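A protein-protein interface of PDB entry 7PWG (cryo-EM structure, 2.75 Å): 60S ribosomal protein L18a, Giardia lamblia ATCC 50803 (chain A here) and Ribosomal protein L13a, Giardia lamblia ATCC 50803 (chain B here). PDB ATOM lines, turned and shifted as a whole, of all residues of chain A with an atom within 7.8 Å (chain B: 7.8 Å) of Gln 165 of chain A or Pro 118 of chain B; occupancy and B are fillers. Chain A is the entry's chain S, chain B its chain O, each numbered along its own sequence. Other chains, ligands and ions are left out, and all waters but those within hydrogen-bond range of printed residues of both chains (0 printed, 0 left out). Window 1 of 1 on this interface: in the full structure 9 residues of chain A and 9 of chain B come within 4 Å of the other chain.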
ATOM      1  N   VAL A 155     -26.688  13.341  -2.351  1.00  0.00           N
ATOM      2  CA  VAL A 155     -25.459  13.913  -2.890  1.00  0.00           C
ATOM      3  C   VAL A 155     -25.767  15.071  -3.830  1.00  0.00           C
ATOM      4  O   VAL A 155     -25.097  16.109  -3.792  1.00  0.00           O
ATOM      5  CB  VAL A 155     -24.618  12.826  -3.583  1.00  0.00           C
ATOM      6  CG1 VAL A 155     -23.208  13.315  -3.830  1.00  0.00           C
ATOM      7  CG2 VAL A 155     -24.586  11.572  -2.759  1.00  0.00           C
ATOM      8  N   LYS A 156     -26.780  14.909  -4.684  1.00  0.00           N
ATOM      9  CA  LYS A 156     -27.154  15.958  -5.627  1.00  0.00           C
ATOM     10  C   LYS A 156     -27.573  17.231  -4.914  1.00  0.00           C
ATOM     11  O   LYS A 156     -27.254  18.334  -5.361  1.00  0.00           O
ATOM     12  CB  LYS A 156     -28.305  15.500  -6.523  1.00  0.00           C
ATOM     13  CG  LYS A 156     -27.965  14.494  -7.546  1.00  0.00           C
ATOM     14  CD  LYS A 156     -29.214  14.032  -8.245  1.00  0.00           C
ATOM     15  CE  LYS A 156     -29.985  15.171  -8.845  1.00  0.00           C
ATOM     16  NZ  LYS A 156     -31.312  14.736  -9.319  1.00  0.00           N
ATOM     17  N   ALA A 158     -26.690  18.503  -2.023  1.00  0.00           N
ATOM     18  CA  ALA A 158     -25.542  19.261  -1.553  1.00  0.00           C
ATOM     19  C   ALA A 158     -24.824  19.965  -2.696  1.00  0.00           C
ATOM     20  O   ALA A 158     -24.203  21.009  -2.484  1.00  0.00           O
ATOM     21  CB  ALA A 158     -24.584  18.342  -0.800  1.00  0.00           C
ATOM     22  N   ALA A 159     -24.907  19.426  -3.904  1.00  0.00           N
ATOM     23  CA  ALA A 159     -24.280  20.004  -5.080  1.00  0.00           C
ATOM     24  C   ALA A 159     -25.092  21.122  -5.699  1.00  0.00           C
ATOM     25  O   ALA A 159     -24.863  21.455  -6.862  1.00  0.00           O
ATOM     26  CB  ALA A 159     -24.018  18.920  -6.126  1.00  0.00           C
ATOM     27  N   ARG A 160     -26.037  21.713  -4.979  1.00  0.00           N
ATOM     28  CA  ARG A 160     -26.762  22.852  -5.520  1.00  0.00           C
ATOM     29  C   ARG A 160     -26.208  24.178  -5.036  1.00  0.00           C
ATOM     30  O   ARG A 160     -26.379  25.188  -5.721  1.00  0.00           O
ATOM     31  CB  ARG A 160     -28.249  22.768  -5.175  1.00  0.00           C
ATOM     32  CG  ARG A 160     -29.101  23.706  -6.010  1.00  0.00           C
ATOM     33  CD  ARG A 160     -30.355  24.151  -5.299  1.00  0.00           C
ATOM     34  NE  ARG A 160     -31.198  23.017  -4.952  1.00  0.00           N
ATOM     35  CZ  ARG A 160     -31.885  22.312  -5.840  1.00  0.00           C
ATOM     36  NH1 ARG A 160     -31.815  22.623  -7.124  1.00  0.00           N
ATOM     37  NH2 ARG A 160     -32.627  21.289  -5.451  1.00  0.00           N
ATOM     38  N   THR A 161     -25.571  24.212  -3.865  1.00  0.00           N
ATOM     39  CA  THR A 161     -24.763  25.360  -3.469  1.00  0.00           C
ATOM     40  C   THR A 161     -23.286  25.130  -3.728  1.00  0.00           C
ATOM     41  O   THR A 161     -22.601  26.026  -4.224  1.00  0.00           O
ATOM     42  CB  THR A 161     -24.974  25.701  -1.989  1.00  0.00           C
ATOM     43  OG1 THR A 161     -24.254  24.777  -1.171  1.00  0.00           O
ATOM     44  CG2 THR A 161     -26.441  25.635  -1.630  1.00  0.00           C
ATOM     45  N   ALA A 162     -22.787  23.930  -3.438  1.00  0.00           N
ATOM     46  CA  ALA A 162     -21.412  23.547  -3.751  1.00  0.00           C
ATOM     47  C   ALA A 162     -21.318  23.190  -5.234  1.00  0.00           C
ATOM     48  O   ALA A 162     -21.154  22.036  -5.629  1.00  0.00           O
ATOM     49  CB  ALA A 162     -20.972  22.389  -2.871  1.00  0.00           C
ATOM     50  N   ARG A 163     -21.395  24.229  -6.062  1.00  0.00           N
ATOM     51  CA  ARG A 163     -21.515  24.039  -7.499  1.00  0.00           C
ATOM     52  C   ARG A 163     -20.245  23.461  -8.120  1.00  0.00           C
ATOM     53  O   ARG A 163     -20.329  22.686  -9.076  1.00  0.00           O
ATOM     54  CB  ARG A 163     -21.887  25.363  -8.152  1.00  0.00           C
ATOM     55  CG  ARG A 163     -21.805  25.350  -9.645  1.00  0.00           C
ATOM     56  CD  ARG A 163     -22.252  26.650 -10.227  1.00  0.00           C
ATOM     57  NE  ARG A 163     -23.689  26.819 -10.127  1.00  0.00           N
ATOM     58  CZ  ARG A 163     -24.417  27.435 -11.043  1.00  0.00           C
ATOM     59  NH1 ARG A 163     -23.836  27.933 -12.123  1.00  0.00           N
ATOM     60  NH2 ARG A 163     -25.723  27.547 -10.880  1.00  0.00           N
ATOM     61  N   PHE A 164     -19.076  23.823  -7.613  1.00  0.00           N
ATOM     62  CA  PHE A 164     -17.809  23.293  -8.102  1.00  0.00           C
ATOM     63  C   PHE A 164     -17.071  22.615  -6.961  1.00  0.00           C
ATOM     64  O   PHE A 164     -17.059  23.117  -5.840  1.00  0.00           O
ATOM     65  CB  PHE A 164     -16.927  24.387  -8.686  1.00  0.00           C
ATOM     66  CG  PHE A 164     -17.578  25.189  -9.766  1.00  0.00           C
ATOM     67  CD1 PHE A 164     -18.341  26.294  -9.463  1.00  0.00           C
ATOM     68  CD2 PHE A 164     -17.415  24.852 -11.087  1.00  0.00           C
ATOM     69  CE1 PHE A 164     -18.920  27.043 -10.454  1.00  0.00           C
ATOM     70  CE2 PHE A 164     -18.002  25.596 -12.075  1.00  0.00           C
ATOM     71  CZ  PHE A 164     -18.753  26.689 -11.759  1.00  0.00           C
ATOM     72  N   GLN A 165     -16.458  21.472  -7.253  1.00  0.00           N
ATOM     73  CA  GLN A 165     -15.779  20.651  -6.261  1.00  0.00           C
ATOM     74  C   GLN A 165     -14.462  20.176  -6.855  1.00  0.00           C
ATOM     75  O   GLN A 165     -14.189  20.396  -8.031  1.00  0.00           O
ATOM     76  CB  GLN A 165     -16.669  19.486  -5.838  1.00  0.00           C
ATOM     77  CG  GLN A 165     -18.000  19.949  -5.300  1.00  0.00           C
ATOM     78  CD  GLN A 165     -18.759  18.868  -4.600  1.00  0.00           C
ATOM     79  OE1 GLN A 165     -18.175  17.940  -4.065  1.00  0.00           O
ATOM     80  NE2 GLN A 165     -20.077  18.973  -4.607  1.00  0.00           N
ATOM     81  N   ASP A 166     -13.632  19.509  -6.059  1.00  0.00           N
ATOM     82  CA  ASP A 166     -12.367  19.030  -6.608  1.00  0.00           C
ATOM     83  C   ASP A 166     -12.343  17.536  -6.927  1.00  0.00           C
ATOM     84  O   ASP A 166     -11.489  17.105  -7.705  1.00  0.00           O
ATOM     85  CB  ASP A 166     -11.198  19.368  -5.676  1.00  0.00           C
ATOM     86  CG  ASP A 166     -11.558  19.254  -4.232  1.00  0.00           C
ATOM     87  OD1 ASP A 166     -12.728  19.522  -3.904  1.00  0.00           O
ATOM     88  OD2 ASP A 166     -10.685  18.897  -3.423  1.00  0.00           O
ATOM     89  N   ARG A 167     -13.250  16.739  -6.379  1.00  0.00           N
ATOM     90  CA  ARG A 167     -13.402  15.356  -6.811  1.00  0.00           C
ATOM     91  C   ARG A 167     -14.881  15.041  -6.934  1.00  0.00           C
ATOM     92  O   ARG A 167     -15.721  15.671  -6.292  1.00  0.00           O
ATOM     93  CB  ARG A 167     -12.752  14.362  -5.840  1.00  0.00           C
ATOM     94  CG  ARG A 167     -13.618  13.994  -4.643  1.00  0.00           C
ATOM     95  CD  ARG A 167     -13.568  15.068  -3.587  1.00  0.00           C
ATOM     96  NE  ARG A 167     -14.590  14.928  -2.559  1.00  0.00           N
ATOM     97  CZ  ARG A 167     -15.836  15.374  -2.679  1.00  0.00           C
ATOM     98  NH1 ARG A 167     -16.215  15.982  -3.784  1.00  0.00           N
ATOM     99  NH2 ARG A 167     -16.702  15.221  -1.692  1.00  0.00           N
ATOM    100  N   ALA A 168     -15.194  14.054  -7.753  1.00  0.00           N
ATOM    101  CA  ALA A 168     -16.573  13.601  -7.855  1.00  0.00           C
ATOM    102  C   ALA A 168     -16.939  12.823  -6.597  1.00  0.00           C
ATOM    103  O   ALA A 168     -16.284  11.823  -6.290  1.00  0.00           O
ATOM    104  CB  ALA A 168     -16.764  12.751  -9.104  1.00  0.00           C
ATOM    105  N   PRO A 169     -17.948  13.246  -5.841  1.00  0.00           N
ATOM    106  CA  PRO A 169     -18.277  12.564  -4.587  1.00  0.00           C
ATOM    107  C   PRO A 169     -18.846  11.171  -4.793  1.00  0.00           C
ATOM    108  O   PRO A 169     -19.408  10.833  -5.837  1.00  0.00           O
ATOM    109  CB  PRO A 169     -19.318  13.490  -3.952  1.00  0.00           C
ATOM    110  CG  PRO A 169     -19.852  14.282  -5.069  1.00  0.00           C
ATOM    111  CD  PRO A 169     -18.712  14.491  -5.988  1.00  0.00           C
ATOM    112  N   HIS A 170     -18.685  10.361  -3.761  1.00  0.00           N
ATOM    113  CA  HIS A 170     -19.192   9.002  -3.688  1.00  0.00           C
ATOM    114  C   HIS A 170     -20.623   8.980  -3.158  1.00  0.00           C
ATOM    115  O   HIS A 170     -21.148   9.974  -2.664  1.00  0.00           O
ATOM    116  CB  HIS A 170     -18.287   8.157  -2.796  1.00  0.00           C
ATOM    117  CG  HIS A 170     -16.989   7.781  -3.435  1.00  0.00           C
ATOM    118  ND1 HIS A 170     -15.944   7.228  -2.730  1.00  0.00           N
ATOM    119  CD2 HIS A 170     -16.570   7.873  -4.717  1.00  0.00           C
ATOM    120  CE1 HIS A 170     -14.942   6.986  -3.555  1.00  0.00           C
ATOM    121  NE2 HIS A 170     -15.295   7.373  -4.764  1.00  0.00           N
ATOM    122  N   VAL B   5     -11.144  25.557 -14.729  1.00  0.00           N
ATOM    123  CA  VAL B   5     -10.819  24.476 -15.653  1.00  0.00           C
ATOM    124  C   VAL B   5     -11.637  23.261 -15.260  1.00  0.00           C
ATOM    125  O   VAL B   5     -11.522  22.767 -14.135  1.00  0.00           O
ATOM    126  CB  VAL B   5      -9.319  24.156 -15.653  1.00  0.00           C
ATOM    127  CG1 VAL B   5      -9.033  23.030 -16.595  1.00  0.00           C
ATOM    128  CG2 VAL B   5      -8.523  25.378 -16.036  1.00  0.00           C
ATOM    129  N   GLY B  10     -17.562  12.388 -17.870  1.00  0.00           N
ATOM    130  CA  GLY B  10     -18.695  11.982 -17.067  1.00  0.00           C
ATOM    131  C   GLY B  10     -19.876  12.926 -17.035  1.00  0.00           C
ATOM    132  O   GLY B  10     -20.890  12.585 -16.425  1.00  0.00           O
ATOM    133  N   HIS B  11     -19.798  14.072 -17.695  1.00  0.00           N
ATOM    134  CA  HIS B  11     -20.795  15.126 -17.595  1.00  0.00           C
ATOM    135  C   HIS B  11     -21.824  15.047 -18.712  1.00  0.00           C
ATOM    136  O   HIS B  11     -21.523  14.630 -19.828  1.00  0.00           O
ATOM    137  CB  HIS B  11     -20.130  16.504 -17.632  1.00  0.00           C
ATOM    138  CG  HIS B  11     -19.355  16.844 -16.401  1.00  0.00           C
ATOM    139  ND1 HIS B  11     -18.171  16.228 -16.074  1.00  0.00           N
ATOM    140  CD2 HIS B  11     -19.583  17.756 -15.431  1.00  0.00           C
ATOM    141  CE1 HIS B  11     -17.711  16.735 -14.945  1.00  0.00           C
ATOM    142  NE2 HIS B  11     -18.546  17.670 -14.541  1.00  0.00           N
ATOM    143  N   ILE B  19     -24.377  25.566 -17.238  1.00  0.00           N
ATOM    144  CA  ILE B  19     -23.513  26.136 -16.206  1.00  0.00           C
ATOM    145  C   ILE B  19     -22.475  27.073 -16.814  1.00  0.00           C
ATOM    146  O   ILE B  19     -22.324  28.215 -16.384  1.00  0.00           O
ATOM    147  CB  ILE B  19     -22.839  25.016 -15.398  1.00  0.00           C
ATOM    148  CG1 ILE B  19     -23.855  24.325 -14.491  1.00  0.00           C
ATOM    149  CG2 ILE B  19     -21.691  25.568 -14.600  1.00  0.00           C
ATOM    150  CD1 ILE B  19     -23.329  23.104 -13.828  1.00  0.00           C
ATOM    151  N   ARG B 114      -7.998  21.352 -11.651  1.00  0.00           N
ATOM    152  CA  ARG B 114      -9.292  21.018 -12.231  1.00  0.00           C
ATOM    153  C   ARG B 114     -10.401  20.940 -11.187  1.00  0.00           C
ATOM    154  O   ARG B 114     -10.154  20.807  -9.988  1.00  0.00           O
ATOM    155  CB  ARG B 114      -9.209  19.692 -12.986  1.00  0.00           C
ATOM    156  CG  ARG B 114      -8.991  19.858 -14.459  1.00  0.00           C
ATOM    157  CD  ARG B 114      -7.526  19.963 -14.791  1.00  0.00           C
ATOM    158  NE  ARG B 114      -6.914  18.646 -14.885  1.00  0.00           N
ATOM    159  CZ  ARG B 114      -5.607  18.431 -14.934  1.00  0.00           C
ATOM    160  NH1 ARG B 114      -4.768  19.448 -14.903  1.00  0.00           N
ATOM    161  NH2 ARG B 114      -5.143  17.196 -15.016  1.00  0.00           N
ATOM    162  N   VAL B 115     -11.647  21.032 -11.670  1.00  0.00           N
ATOM    163  CA  VAL B 115     -12.850  20.892 -10.853  1.00  0.00           C
ATOM    164  C   VAL B 115     -13.902  20.117 -11.638  1.00  0.00           C
ATOM    165  O   VAL B 115     -13.758  19.869 -12.833  1.00  0.00           O
ATOM    166  CB  VAL B 115     -13.433  22.249 -10.408  1.00  0.00           C
ATOM    167  CG1 VAL B 115     -12.522  22.926  -9.427  1.00  0.00           C
ATOM    168  CG2 VAL B 115     -13.709  23.127 -11.597  1.00  0.00           C
ATOM    169  N   VAL B 116     -14.982  19.740 -10.941  1.00  0.00           N
ATOM    170  CA  VAL B 116     -16.117  19.030 -11.527  1.00  0.00           C
ATOM    171  C   VAL B 116     -17.413  19.654 -11.019  1.00  0.00           C
ATOM    172  O   VAL B 116     -17.424  20.413 -10.053  1.00  0.00           O
ATOM    173  CB  VAL B 116     -16.105  17.511 -11.214  1.00  0.00           C
ATOM    174  CG1 VAL B 116     -14.759  16.906 -11.506  1.00  0.00           C
ATOM    175  CG2 VAL B 116     -16.491  17.257  -9.798  1.00  0.00           C
ATOM    176  N   CYS B 117     -18.519  19.323 -11.694  1.00  0.00           N
ATOM    177  CA  CYS B 117     -19.859  19.788 -11.333  1.00  0.00           C
ATOM    178  C   CYS B 117     -20.769  18.579 -11.171  1.00  0.00           C
ATOM    179  O   CYS B 117     -21.442  18.166 -12.122  1.00  0.00           O
ATOM    180  CB  CYS B 117     -20.428  20.742 -12.382  1.00  0.00           C
ATOM    181  SG  CYS B 117     -19.398  22.142 -12.839  1.00  0.00           S
ATOM    182  N   PRO B 118     -20.821  17.986  -9.979  1.00  0.00           N
ATOM    183  CA  PRO B 118     -21.558  16.723  -9.822  1.00  0.00           C
ATOM    184  C   PRO B 118     -23.057  16.815 -10.069  1.00  0.00           C
ATOM    185  O   PRO B 118     -23.673  15.787 -10.352  1.00  0.00           O
ATOM    186  CB  PRO B 118     -21.243  16.314  -8.378  1.00  0.00           C
ATOM    187  CG  PRO B 118     -20.678  17.505  -7.744  1.00  0.00           C
ATOM    188  CD  PRO B 118     -20.064  18.340  -8.770  1.00  0.00           C
ATOM    189  N   SER B 119     -23.668  17.991  -9.987  1.00  0.00           N
ATOM    190  CA  SER B 119     -25.088  18.092 -10.289  1.00  0.00           C
ATOM    191  C   SER B 119     -25.401  17.862 -11.765  1.00  0.00           C
ATOM    192  O   SER B 119     -26.574  17.720 -12.117  1.00  0.00           O
ATOM    193  CB  SER B 119     -25.612  19.454  -9.838  1.00  0.00           C
ATOM    194  OG  SER B 119     -24.594  20.432  -9.916  1.00  0.00           O
ATOM    195  N   ALA B 120     -24.388  17.826 -12.627  1.00  0.00           N
ATOM    196  CA  ALA B 120     -24.559  17.563 -14.048  1.00  0.00           C
ATOM    197  C   ALA B 120     -23.754  16.361 -14.514  1.00  0.00           C
ATOM    198  O   ALA B 120     -23.442  16.260 -15.698  1.00  0.00           O
ATOM    199  CB  ALA B 120     -24.181  18.791 -14.866  1.00  0.00           C
ATOM    200  N   MET B 121     -23.412  15.449 -13.616  1.00  0.00           N
ATOM    201  CA  MET B 121     -22.687  14.238 -13.967  1.00  0.00           C
ATOM    202  C   MET B 121     -23.662  13.076 -14.087  1.00  0.00           C
ATOM    203  O   MET B 121     -24.578  12.946 -13.278  1.00  0.00           O
ATOM    204  CB  MET B 121     -21.606  13.932 -12.929  1.00  0.00           C
ATOM    205  CG  MET B 121     -20.407  14.833 -13.011  1.00  0.00           C
ATOM    206  SD  MET B 121     -19.154  14.558 -11.741  1.00  0.00           S
ATOM    207  CE  MET B 121     -18.117  13.369 -12.568  1.00  0.00           C
ATOM    208  N   ALA B 122     -23.449  12.222 -15.098  1.00  0.00           N
ATOM    209  CA  ALA B 122     -24.449  11.221 -15.473  1.00  0.00           C
ATOM    210  C   ALA B 122     -24.694  10.178 -14.389  1.00  0.00           C
ATOM    211  O   ALA B 122     -25.806   9.654 -14.296  1.00  0.00           O
ATOM    212  CB  ALA B 122     -24.050  10.515 -16.772  1.00  0.00           C
ATOM    213  N   TYR B 123     -23.695   9.849 -13.567  1.00  0.00           N
ATOM    214  CA  TYR B 123     -23.922   8.864 -12.514  1.00  0.00           C
ATOM    215  C   TYR B 123     -24.839   9.385 -11.414  1.00  0.00           C
ATOM    216  O   TYR B 123     -25.360   8.595 -10.625  1.00  0.00           O
ATOM    217  CB  TYR B 123     -22.586   8.391 -11.933  1.00  0.00           C
ATOM    218  CG  TYR B 123     -21.983   9.269 -10.876  1.00  0.00           C
ATOM    219  CD1 TYR B 123     -21.313  10.431 -11.212  1.00  0.00           C
ATOM    220  CD2 TYR B 123     -22.078   8.935  -9.540  1.00  0.00           C
ATOM    221  CE1 TYR B 123     -20.778  11.235 -10.256  1.00  0.00           C
ATOM    222  CE2 TYR B 123     -21.535   9.747  -8.570  1.00  0.00           C
ATOM    223  CZ  TYR B 123     -20.887  10.889  -8.938  1.00  0.00           C
ATOM    224  OH  TYR B 123     -20.335  11.699  -7.983  1.00  0.00           O
ATOM    225  N   LEU B 124     -25.040  10.696 -11.330  1.00  0.00           N
ATOM    226  CA  LEU B 124     -26.000  11.250 -10.395  1.00  0.00           C
ATOM    227  C   LEU B 124     -27.291  11.681 -11.065  1.00  0.00           C
ATOM    228  O   LEU B 124     -28.310  11.796 -10.381  1.00  0.00           O
ATOM    229  CB  LEU B 124     -25.390  12.443  -9.656  1.00  0.00           C
ATOM    230  CG  LEU B 124     -24.375  12.171  -8.552  1.00  0.00           C
ATOM    231  CD1 LEU B 124     -23.943  13.470  -7.939  1.00  0.00           C
ATOM    232  CD2 LEU B 124     -24.932  11.256  -7.492  1.00  0.00           C
ATOM    233  N   CYS B 125     -27.276  11.872 -12.384  1.00  0.00           N
ATOM    234  CA  CYS B 125     -28.365  12.443 -13.165  1.00  0.00           C
ATOM    235  C   CYS B 125     -29.273  11.408 -13.810  1.00  0.00           C
ATOM    236  O   CYS B 125     -30.483  11.615 -13.861  1.00  0.00           O
ATOM    237  CB  CYS B 125     -27.802  13.346 -14.270  1.00  0.00           C
ATOM    238  SG  CYS B 125     -27.588  15.072 -13.846  1.00  0.00           S
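The side-chain hydroxyl (OH) of Tyr 123 of chain B is in hydrogen-bond range of the backbone carbonyl oxygen (O) of Pro 169 of chain A, 2.5 Å away.
The backbone NH (N) of Val 116 of chain B sits at hydrogen-bond distance from the backbone carbonyl oxygen (O) of Gln 165 of chain A.
OG of Ser 119 of chain B lies within hydrogen-bond range of O of Ala 159 of chain A (3.2 Å).
OE1 of Gln 165 of chain A lies within hydrogen-bond range of NH1 of Arg 167 of chain A.
The side-chain sulfur (SG) of Cys 125 of chain B sits close to the backbone carbonyl oxygen (O) of Met 121 of chain B (3.7 Å).
NE2 of Gln 165 of chain A is in hydrogen-bond range of O of Ala 162 of chain A.
The backbone carbonyl oxygen (O) of Val 5 of chain B is in hydrogen-bond range of the backbone NH (N) of Val 115 of chain B (3.0 Å).
NE2 of His 11 of chain B lies within hydrogen-bond range of N of Cys 117 of chain B (3.3 Å).
The backbone carbonyl oxygen of Ser 119 of chain B lies within hydrogen-bond range of the side-chain sulfur of Cys 125 of chain B.
Among the printed residues, pairs that only touch across the chains: Lys 156 of chain A with Leu 124 of chain B, Ala 159 of chain A with Pro 118 of chain B, Arg 163 of chain A with Val 116 of chain B, Arg 163 of chain A with Cys 117 of chain B, Phe 164 of chain A with Val 116 of chain B, Phe 164 of chain A with Cys 117 of chain B, Gln 165 of chain A with Val 115 of chain B, Gln 165 of chain A with Pro 118 of chain B, Arg 167 of chain A with Val 116 of chain B, Ala 168 of chain A with Met 121 of chain B, Ala 168 of chain A with Tyr 123 of chain B and Pro 169 of chain A with Pro 118 of chain B.
Of the printed residues of chain B, Ala 159 of chain A touches Pro 118 (3.97 Å) and Ser 119 (3.2 Å).
Thr 161 of chain A touches none of the printed residues of chain B.
Gln 165 of chain A touches just these residues of chain B: Val 115 (3.1 Å), Val 116 (3.1 Å) and Pro 118 (3.5 Å).
Of the printed residues of chain A, Val 116 of chain B touches Arg 163, Phe 164, Gln 165 and Arg 167.
Pro 118 of chain B touches three residues of chain A.
Ala 122 of chain B touches none of the printed residues of chain A.
The nearest residue of chain B that does not touch Gln 165 of chain A is Arg 114 of chain B (4.5 Å).
The nearest printed residue of chain B that does not touch Phe 164 of chain A is Val 115 of chain B (4.1 Å).
Of the 15 printed residues of chain A, 8 touch a printed residue of chain B.
Of the 16 printed residues of chain B, 8 touch a printed residue of chain A.
Among the printed residues, 15 pairs touch across the chains.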
